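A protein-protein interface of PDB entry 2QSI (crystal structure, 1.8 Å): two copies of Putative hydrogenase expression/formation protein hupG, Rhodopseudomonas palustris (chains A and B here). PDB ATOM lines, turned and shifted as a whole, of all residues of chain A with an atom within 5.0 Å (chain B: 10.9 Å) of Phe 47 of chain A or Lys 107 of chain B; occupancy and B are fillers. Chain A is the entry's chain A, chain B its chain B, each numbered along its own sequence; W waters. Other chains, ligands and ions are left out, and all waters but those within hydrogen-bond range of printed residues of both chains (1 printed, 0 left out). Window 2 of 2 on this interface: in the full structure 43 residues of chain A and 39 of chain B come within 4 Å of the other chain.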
ATOM      1  N   ARG A  41      29.910   5.368  19.219  1.00  0.00           N
ATOM      2  CA  ARG A  41      30.748   4.691  20.191  1.00  0.00           C
ATOM      3  C   ARG A  41      30.387   5.099  21.606  1.00  0.00           C
ATOM      4  O   ARG A  41      29.766   4.334  22.334  1.00  0.00           O
ATOM      5  CB  ARG A  41      32.248   4.975  19.896  1.00  0.00           C
ATOM      6  CG  ARG A  41      33.183   4.281  20.886  1.00  0.00           C
ATOM      7  CD  ARG A  41      34.610   4.793  20.799  1.00  0.00           C
ATOM      8  NE  ARG A  41      35.321   4.403  19.574  1.00  0.00           N
ATOM      9  CZ  ARG A  41      36.033   3.285  19.395  1.00  0.00           C
ATOM     10  NH1 ARG A  41      36.183   2.394  20.370  1.00  0.00           N
ATOM     11  NH2 ARG A  41      36.635   3.109  18.230  1.00  0.00           N
ATOM     12  N   GLY A  42      30.746   6.328  21.976  1.00  0.00           N
ATOM     13  CA  GLY A  42      30.583   6.795  23.331  1.00  0.00           C
ATOM     14  C   GLY A  42      31.846   6.808  24.175  1.00  0.00           C
ATOM     15  O   GLY A  42      32.857   6.169  23.865  1.00  0.00           O
ATOM     16  N   ASP A  43      31.761   7.523  25.282  1.00  0.00           N
ATOM     17  CA  ASP A  43      32.869   7.611  26.240  1.00  0.00           C
ATOM     18  C   ASP A  43      33.295   6.237  26.748  1.00  0.00           C
ATOM     19  O   ASP A  43      32.448   5.376  26.989  1.00  0.00           O
ATOM     20  CB  ASP A  43      32.424   8.484  27.425  1.00  0.00           C
ATOM     21  CG  ASP A  43      33.438   8.515  28.519  1.00  0.00           C
ATOM     22  OD1 ASP A  43      34.490   9.160  28.315  1.00  0.00           O
ATOM     23  OD2 ASP A  43      33.182   7.891  29.568  1.00  0.00           O
ATOM     24  N   ALA A  44      34.612   6.045  26.900  1.00  0.00           N
ATOM     25  CA  ALA A  44      35.232   4.760  27.300  1.00  0.00           C
ATOM     26  C   ALA A  44      34.880   4.356  28.730  1.00  0.00           C
ATOM     27  O   ALA A  44      34.879   3.180  29.031  1.00  0.00           O
ATOM     28  CB  ALA A  44      36.765   4.850  27.186  1.00  0.00           C
ATOM     29  N   VAL A  45      34.626   5.323  29.599  1.00  0.00           N
ATOM     30  CA  VAL A  45      34.296   5.043  31.015  1.00  0.00           C
ATOM     31  C   VAL A  45      32.829   4.622  31.135  1.00  0.00           C
ATOM     32  O   VAL A  45      32.511   3.646  31.798  1.00  0.00           O
ATOM     33  CB  VAL A  45      34.596   6.264  31.945  1.00  0.00           C
ATOM     34  CG1 VAL A  45      34.423   5.868  33.430  1.00  0.00           C
ATOM     35  CG2 VAL A  45      36.019   6.791  31.717  1.00  0.00           C
ATOM     36  N   ARG A  46      31.948   5.345  30.451  1.00  0.00           N
ATOM     37  CA  ARG A  46      30.535   5.010  30.456  1.00  0.00           C
ATOM     38  C   ARG A  46      30.181   3.811  29.597  1.00  0.00           C
ATOM     39  O   ARG A  46      29.291   3.035  29.972  1.00  0.00           O
ATOM     40  CB  ARG A  46      29.705   6.187  29.996  1.00  0.00           C
ATOM     41  CG  ARG A  46      29.752   7.394  30.881  1.00  0.00           C
ATOM     42  CD  ARG A  46      29.000   8.542  30.199  1.00  0.00           C
ATOM     43  NE  ARG A  46      27.558   8.311  30.238  1.00  0.00           N
ATOM     44  CZ  ARG A  46      26.668   8.882  29.430  1.00  0.00           C
ATOM     45  NH1 ARG A  46      27.056   9.729  28.479  1.00  0.00           N
ATOM     46  NH2 ARG A  46      25.372   8.596  29.578  1.00  0.00           N
ATOM     47  N   PHE A  47      30.867   3.668  28.446  1.00  0.00           N
ATOM     48  CA  PHE A  47      30.572   2.632  27.442  1.00  0.00           C
ATOM     49  C   PHE A  47      31.848   1.881  26.987  1.00  0.00           C
ATOM     50  O   PHE A  47      32.200   1.843  25.781  1.00  0.00           O
ATOM     51  CB  PHE A  47      29.923   3.281  26.220  1.00  0.00           C
ATOM     52  CG  PHE A  47      28.728   4.131  26.548  1.00  0.00           C
ATOM     53  CD1 PHE A  47      27.504   3.552  26.846  1.00  0.00           C
ATOM     54  CD2 PHE A  47      28.816   5.508  26.563  1.00  0.00           C
ATOM     55  CE1 PHE A  47      26.397   4.340  27.145  1.00  0.00           C
ATOM     56  CE2 PHE A  47      27.708   6.292  26.888  1.00  0.00           C
ATOM     57  CZ  PHE A  47      26.510   5.703  27.158  1.00  0.00           C
ATOM     58  N   PRO A  48      32.529   1.245  27.938  1.00  0.00           N
ATOM     59  CA  PRO A  48      33.790   0.585  27.568  1.00  0.00           C
ATOM     60  C   PRO A  48      33.575  -0.551  26.549  1.00  0.00           C
ATOM     61  O   PRO A  48      34.430  -0.797  25.687  1.00  0.00           O
ATOM     62  CB  PRO A  48      34.313   0.045  28.904  1.00  0.00           C
ATOM     63  CG  PRO A  48      33.140  -0.073  29.763  1.00  0.00           C
ATOM     64  CD  PRO A  48      32.208   1.056  29.374  1.00  0.00           C
ATOM     65  N   GLU A  49      32.405  -1.173  26.603  1.00  0.00           N
ATOM     66  CA  GLU A  49      32.058  -2.272  25.682  1.00  0.00           C
ATOM     67  C   GLU A  49      31.905  -1.814  24.222  1.00  0.00           C
ATOM     68  O   GLU A  49      31.876  -2.657  23.313  1.00  0.00           O
ATOM     69  CB  GLU A  49      30.779  -2.982  26.162  1.00  0.00           C
ATOM     70  CG  GLU A  49      29.476  -2.211  25.914  1.00  0.00           C
ATOM     71  CD  GLU A  49      29.180  -1.069  26.874  1.00  0.00           C
ATOM     72  OE1 GLU A  49      29.966  -0.777  27.844  1.00  0.00           O
ATOM     73  OE2 GLU A  49      28.099  -0.485  26.655  1.00  0.00           O
ATOM     74  N   ALA A  50      31.794  -0.500  23.991  1.00  0.00           N
ATOM     75  CA  ALA A  50      31.753   0.062  22.629  1.00  0.00           C
ATOM     76  C   ALA A  50      33.005  -0.305  21.846  1.00  0.00           C
ATOM     77  O   ALA A  50      32.962  -0.486  20.637  1.00  0.00           O
ATOM     78  CB  ALA A  50      31.562   1.580  22.657  1.00  0.00           C
ATOM     79  N   ALA A  51      34.120  -0.442  22.532  1.00  0.00           N
ATOM     80  CA  ALA A  51      35.349  -0.908  21.868  1.00  0.00           C
ATOM     81  C   ALA A  51      35.185  -2.316  21.256  1.00  0.00           C
ATOM     82  O   ALA A  51      35.824  -2.650  20.257  1.00  0.00           O
ATOM     83  CB  ALA A  51      36.544  -0.880  22.849  1.00  0.00           C
ATOM     84  N   VAL A  89      20.415   5.419  21.854  1.00  0.00           N
ATOM     85  CA  VAL A  89      21.454   5.166  22.857  1.00  0.00           C
ATOM     86  C   VAL A  89      22.804   4.806  22.218  1.00  0.00           C
ATOM     87  O   VAL A  89      22.872   4.504  21.024  1.00  0.00           O
ATOM     88  CB  VAL A  89      21.006   4.016  23.806  1.00  0.00           C
ATOM     89  CG1 VAL A  89      19.689   4.365  24.483  1.00  0.00           C
ATOM     90  CG2 VAL A  89      20.900   2.678  23.056  1.00  0.00           C
ATOM     91  N   CYS A  90      23.877   4.854  23.005  1.00  0.00           N
ATOM     92  CA  CYS A  90      25.181   4.391  22.568  1.00  0.00           C
ATOM     93  C   CYS A  90      25.602   3.202  23.412  1.00  0.00           C
ATOM     94  O   CYS A  90      25.093   3.003  24.513  1.00  0.00           O
ATOM     95  CB  CYS A  90      26.256   5.480  22.679  1.00  0.00           C
ATOM     96  SG  CYS A  90      25.773   6.902  21.756  1.00  0.00           S
ATOM     97  N   PRO A  91      26.452   2.344  22.861  1.00  0.00           N
ATOM     98  CA  PRO A  91      26.878   2.313  21.456  1.00  0.00           C
ATOM     99  C   PRO A  91      25.739   1.790  20.569  1.00  0.00           C
ATOM    100  O   PRO A  91      24.853   1.065  21.050  1.00  0.00           O
ATOM    101  CB  PRO A  91      28.069   1.350  21.459  1.00  0.00           C
ATOM    102  CG  PRO A  91      27.867   0.495  22.676  1.00  0.00           C
ATOM    103  CD  PRO A  91      27.021   1.244  23.656  1.00  0.00           C
ATOM    104  N   SER A  92      25.741   2.205  19.309  1.00  0.00           N
ATOM    105  CA  SER A  92      24.803   1.754  18.303  1.00  0.00           C
ATOM    106  C   SER A  92      25.486   1.750  16.925  1.00  0.00           C
ATOM    107  O   SER A  92      26.433   2.489  16.701  1.00  0.00           O
ATOM    108  CB  SER A  92      23.576   2.714  18.204  1.00  0.00           C
ATOM    109  OG  SER A  92      22.668   2.540  19.287  1.00  0.00           O
ATOM    110  N   GLY B 103      17.813   1.019   9.661  1.00  0.00           N
ATOM    111  CA  GLY B 103      17.656   0.452  10.976  1.00  0.00           C
ATOM    112  C   GLY B 103      18.768   0.876  11.923  1.00  0.00           C
ATOM    113  O   GLY B 103      19.773   1.442  11.530  1.00  0.00           O
ATOM    114  N   VAL B 104      18.541   0.620  13.201  1.00  0.00           N
ATOM    115  CA  VAL B 104      19.518   0.939  14.212  1.00  0.00           C
ATOM    116  C   VAL B 104      19.702  -0.302  15.072  1.00  0.00           C
ATOM    117  O   VAL B 104      18.710  -0.966  15.497  1.00  0.00           O
ATOM    118  CB  VAL B 104      19.091   2.139  15.069  1.00  0.00           C
ATOM    119  CG1 VAL B 104      20.094   2.394  16.196  1.00  0.00           C
ATOM    120  CG2 VAL B 104      18.914   3.389  14.223  1.00  0.00           C
ATOM    121  N   ILE B 105      20.960  -0.635  15.343  1.00  0.00           N
ATOM    122  CA  ILE B 105      21.283  -1.765  16.207  1.00  0.00           C
ATOM    123  C   ILE B 105      21.937  -1.298  17.503  1.00  0.00           C
ATOM    124  O   ILE B 105      23.109  -0.922  17.518  1.00  0.00           O
ATOM    125  CB  ILE B 105      22.219  -2.764  15.502  1.00  0.00           C
ATOM    126  CG1 ILE B 105      21.625  -3.194  14.158  1.00  0.00           C
ATOM    127  CG2 ILE B 105      22.473  -3.972  16.389  1.00  0.00           C
ATOM    128  CD1 ILE B 105      22.488  -4.175  13.396  1.00  0.00           C
ATOM    129  N   ALA B 106      21.172  -1.325  18.589  1.00  0.00           N
ATOM    130  CA  ALA B 106      21.510  -0.562  19.785  1.00  0.00           C
ATOM    131  C   ALA B 106      22.218  -1.436  20.815  1.00  0.00           C
ATOM    132  O   ALA B 106      21.775  -2.546  21.110  1.00  0.00           O
ATOM    133  CB  ALA B 106      20.261   0.064  20.386  1.00  0.00           C
ATOM    134  N   LYS B 107      23.319  -0.928  21.358  1.00  0.00           N
ATOM    135  CA  LYS B 107      24.075  -1.649  22.375  1.00  0.00           C
ATOM    136  C   LYS B 107      24.820  -2.835  21.771  1.00  0.00           C
ATOM    137  O   LYS B 107      24.619  -3.178  20.605  1.00  0.00           O
ATOM    138  CB  LYS B 107      23.148  -2.126  23.494  1.00  0.00           C
ATOM    139  CG  LYS B 107      22.515  -1.002  24.298  1.00  0.00           C
ATOM    140  CD  LYS B 107      23.567  -0.034  24.815  1.00  0.00           C
ATOM    141  CE  LYS B 107      23.039   0.782  25.983  1.00  0.00           C
ATOM    142  NZ  LYS B 107      23.976   1.875  26.366  1.00  0.00           N
ATOM    143  N   ILE B 108      25.679  -3.457  22.570  1.00  0.00           N
ATOM    144  CA  ILE B 108      26.561  -4.509  22.077  1.00  0.00           C
ATOM    145  C   ILE B 108      25.811  -5.827  21.917  1.00  0.00           C
ATOM    146  O   ILE B 108      25.174  -6.307  22.854  1.00  0.00           O
ATOM    147  CB  ILE B 108      27.763  -4.724  23.016  1.00  0.00           C
ATOM    148  CG1 ILE B 108      28.810  -5.616  22.345  1.00  0.00           C
ATOM    149  CG2 ILE B 108      27.308  -5.327  24.335  1.00  0.00           C
ATOM    150  CD1 ILE B 108      29.573  -4.932  21.233  1.00  0.00           C
ATOM    151  N   GLN B 109      25.892  -6.407  20.723  1.00  0.00           N
ATOM    152  CA  GLN B 109      25.106  -7.608  20.391  1.00  0.00           C
ATOM    153  C   GLN B 109      26.104  -8.672  19.926  1.00  0.00           C
ATOM    154  O   GLN B 109      27.265  -8.344  19.724  1.00  0.00           O
ATOM    155  CB  GLN B 109      24.058  -7.320  19.294  1.00  0.00           C
ATOM    156  CG  GLN B 109      23.077  -6.132  19.572  1.00  0.00           C
ATOM    157  CD  GLN B 109      22.218  -6.309  20.828  1.00  0.00           C
ATOM    158  OE1 GLN B 109      21.915  -7.432  21.214  1.00  0.00           O
ATOM    159  NE2 GLN B 109      21.809  -5.193  21.460  1.00  0.00           N
ATOM    160  N   ASP B 110      25.687  -9.938  19.807  1.00  0.00           N
ATOM    161  CA  ASP B 110      26.588 -10.963  19.265  1.00  0.00           C
ATOM    162  C   ASP B 110      26.689 -10.917  17.742  1.00  0.00           C
ATOM    163  O   ASP B 110      25.859 -10.308  17.065  1.00  0.00           O
ATOM    164  CB  ASP B 110      26.272 -12.388  19.747  1.00  0.00           C
ATOM    165  CG  ASP B 110      24.810 -12.730  19.698  1.00  0.00           C
ATOM    166  OD1 ASP B 110      24.215 -12.646  18.591  1.00  0.00           O
ATOM    167  OD2 ASP B 110      24.270 -13.137  20.775  1.00  0.00           O
ATOM    168  N   TRP B 111      27.713 -11.602  17.235  1.00  0.00           N
ATOM    169  CA  TRP B 111      28.114 -11.595  15.820  1.00  0.00           C
ATOM    170  C   TRP B 111      27.033 -12.099  14.895  1.00  0.00           C
ATOM    171  O   TRP B 111      26.781 -11.494  13.846  1.00  0.00           O
ATOM    172  CB  TRP B 111      29.401 -12.422  15.660  1.00  0.00           C
ATOM    173  CG  TRP B 111      29.891 -12.787  14.295  1.00  0.00           C
ATOM    174  CD1 TRP B 111      30.001 -14.049  13.791  1.00  0.00           C
ATOM    175  CD2 TRP B 111      30.412 -11.908  13.281  1.00  0.00           C
ATOM    176  NE1 TRP B 111      30.521 -14.011  12.517  1.00  0.00           N
ATOM    177  CE2 TRP B 111      30.797 -12.714  12.184  1.00  0.00           C
ATOM    178  CE3 TRP B 111      30.591 -10.523  13.193  1.00  0.00           C
ATOM    179  CZ2 TRP B 111      31.351 -12.184  11.012  1.00  0.00           C
ATOM    180  CZ3 TRP B 111      31.125  -9.990  12.025  1.00  0.00           C
ATOM    181  CH2 TRP B 111      31.497 -10.825  10.942  1.00  0.00           C
ATOM    182  N   SER B 113      23.896 -12.062  15.527  1.00  0.00           N
ATOM    183  CA  SER B 113      22.807 -11.101  15.644  1.00  0.00           C
ATOM    184  C   SER B 113      23.049  -9.903  14.728  1.00  0.00           C
ATOM    185  O   SER B 113      22.141  -9.481  14.033  1.00  0.00           O
ATOM    186  CB  SER B 113      22.590 -10.652  17.096  1.00  0.00           C
ATOM    187  OG  SER B 113      21.527  -9.692  17.180  1.00  0.00           O
ATOM    188  N   TYR B 114      24.271  -9.380  14.706  1.00  0.00           N
ATOM    189  CA  TYR B 114      24.631  -8.324  13.747  1.00  0.00           C
ATOM    190  C   TYR B 114      24.458  -8.776  12.291  1.00  0.00           C
ATOM    191  O   TYR B 114      23.820  -8.087  11.485  1.00  0.00           O
ATOM    192  CB  TYR B 114      26.064  -7.857  13.958  1.00  0.00           C
ATOM    193  CG  TYR B 114      26.242  -6.944  15.131  1.00  0.00           C
ATOM    194  CD1 TYR B 114      25.690  -5.667  15.137  1.00  0.00           C
ATOM    195  CD2 TYR B 114      26.986  -7.339  16.236  1.00  0.00           C
ATOM    196  CE1 TYR B 114      25.847  -4.826  16.208  1.00  0.00           C
ATOM    197  CE2 TYR B 114      27.154  -6.503  17.307  1.00  0.00           C
ATOM    198  CZ  TYR B 114      26.596  -5.239  17.294  1.00  0.00           C
ATOM    199  OH  TYR B 114      26.764  -4.421  18.389  1.00  0.00           O
ATOM    200  N   GLN B 117      20.615  -9.183  11.404  1.00  0.00           N
ATOM    201  CA  GLN B 117      19.942  -7.901  11.312  1.00  0.00           C
ATOM    202  C   GLN B 117      20.409  -7.113  10.097  1.00  0.00           C
ATOM    203  O   GLN B 117      19.587  -6.543   9.413  1.00  0.00           O
ATOM    204  CB  GLN B 117      20.117  -7.064  12.567  1.00  0.00           C
ATOM    205  CG  GLN B 117      19.438  -7.676  13.803  1.00  0.00           C
ATOM    206  CD  GLN B 117      19.521  -6.770  14.996  1.00  0.00           C
ATOM    207  OE1 GLN B 117      19.000  -5.647  14.976  1.00  0.00           O
ATOM    208  NE2 GLN B 117      20.151  -7.251  16.061  1.00  0.00           N
ATOM    209  N   ILE B 118      21.701  -7.067   9.818  1.00  0.00           N
ATOM    210  CA  ILE B 118      22.176  -6.355   8.613  1.00  0.00           C
ATOM    211  C   ILE B 118      21.679  -7.007   7.326  1.00  0.00           C
ATOM    212  O   ILE B 118      21.212  -6.306   6.372  1.00  0.00           O
ATOM    213  CB  ILE B 118      23.704  -6.220   8.612  1.00  0.00           C
ATOM    214  CG1 ILE B 118      24.101  -5.335   9.797  1.00  0.00           C
ATOM    215  CG2 ILE B 118      24.175  -5.622   7.260  1.00  0.00           C
ATOM    216  CD1 ILE B 118      25.549  -5.305  10.148  1.00  0.00           C
HETATM  217  O   HOH W   1      26.099   0.499  28.052  1.00  0.00           O
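Phe 47 of chain A touches one residue of chain B. No residue of chain B comes within 4 Å of Gly 42 of chain A. No residue of chain B comes within 4 Å of Pro 48 of chain A. Printed residues of chain B within 4 Å of Glu 49 of chain A: Ile 108. No residue of chain B comes within 4 Å of Ala 50 of chain A. Of chain B, only Ala 106 comes within 4 Å of Val 89 of chain A. Ser 92 of chain A touches just these residues of chain B: Ile 105 (3.3 Å) and Ala 106 (3.3 Å). Of the printed residues of chain A, Ile 108 of chain B touches Glu 49. Of the printed residues of chain A, Ala 106 of chain B touches Val 89, Pro 91 and Ser 92. Of the printed residues of chain A, Ile 105 of chain B touches Ser 92 (3.3 Å). Trp 111 of chain B touches none of the printed residues of chain A. The nearest residue of chain B that does not touch Phe 47 of chain A is Ile 108 of chain B (8.4 Å). The nearest printed residue of chain A that does not touch Lys 107 of chain B is Val 89 of chain A (4.1 Å).
The backbone carbonyl oxygen (O) of Val 89 of chain A is in hydrogen-bond range of the side-chain hydroxyl (OG) of Ser 92 of chain A, at 2.6 Å. The backbone carbonyl oxygen of Ala 106 of chain B sits at hydrogen-bond distance from the side-chain amide nitrogen of Gln 109 of chain B (2.7 Å). The side-chain hydroxyl (OH) of Tyr 114 of chain B is in hydrogen-bond range of the backbone carbonyl oxygen (O) of Lys 107 of chain B (3.3 Å).
Among the printed residues, merely in contact across the chains: Phe 47 of chain A with Lys 107 of chain B, Glu 49 of chain A with Ile 108 of chain B, Val 89 of chain A with Ala 106 of chain B, Pro 91 of chain A with Ala 106 of chain B, Ser 92 of chain A with Ile 105 of chain B and Ser 92 of chain A with Ala 106 of chain B.
Hydrophobic or aromatic side chains of chain A within 4 Å of the printed part of chain B: Phe 47, Val 89 and Pro 91.
Water W1 lies within hydrogen-bond range of the side-chain carboxylate (OE2) of Glu 49 of chain A and the side-chain amino group (NZ) of Lys 107 of chain B.
No position is printed for both chains. Of the 8 pairs that touch across the chains among the printed residues, none has its exchanged pair printed and touching as well.
The side-chain amino group (NZ) of Lys 107 of chain B lies within hydrogen-bond range of the backbone carbonyl oxygen (O) of Cys 90 of chain A (2.4 Å). The backbone NH (N) of Lys 107 of chain B sits at hydrogen-bond distance from the backbone carbonyl oxygen (O) of Pro 91 of chain A (2.5 Å).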
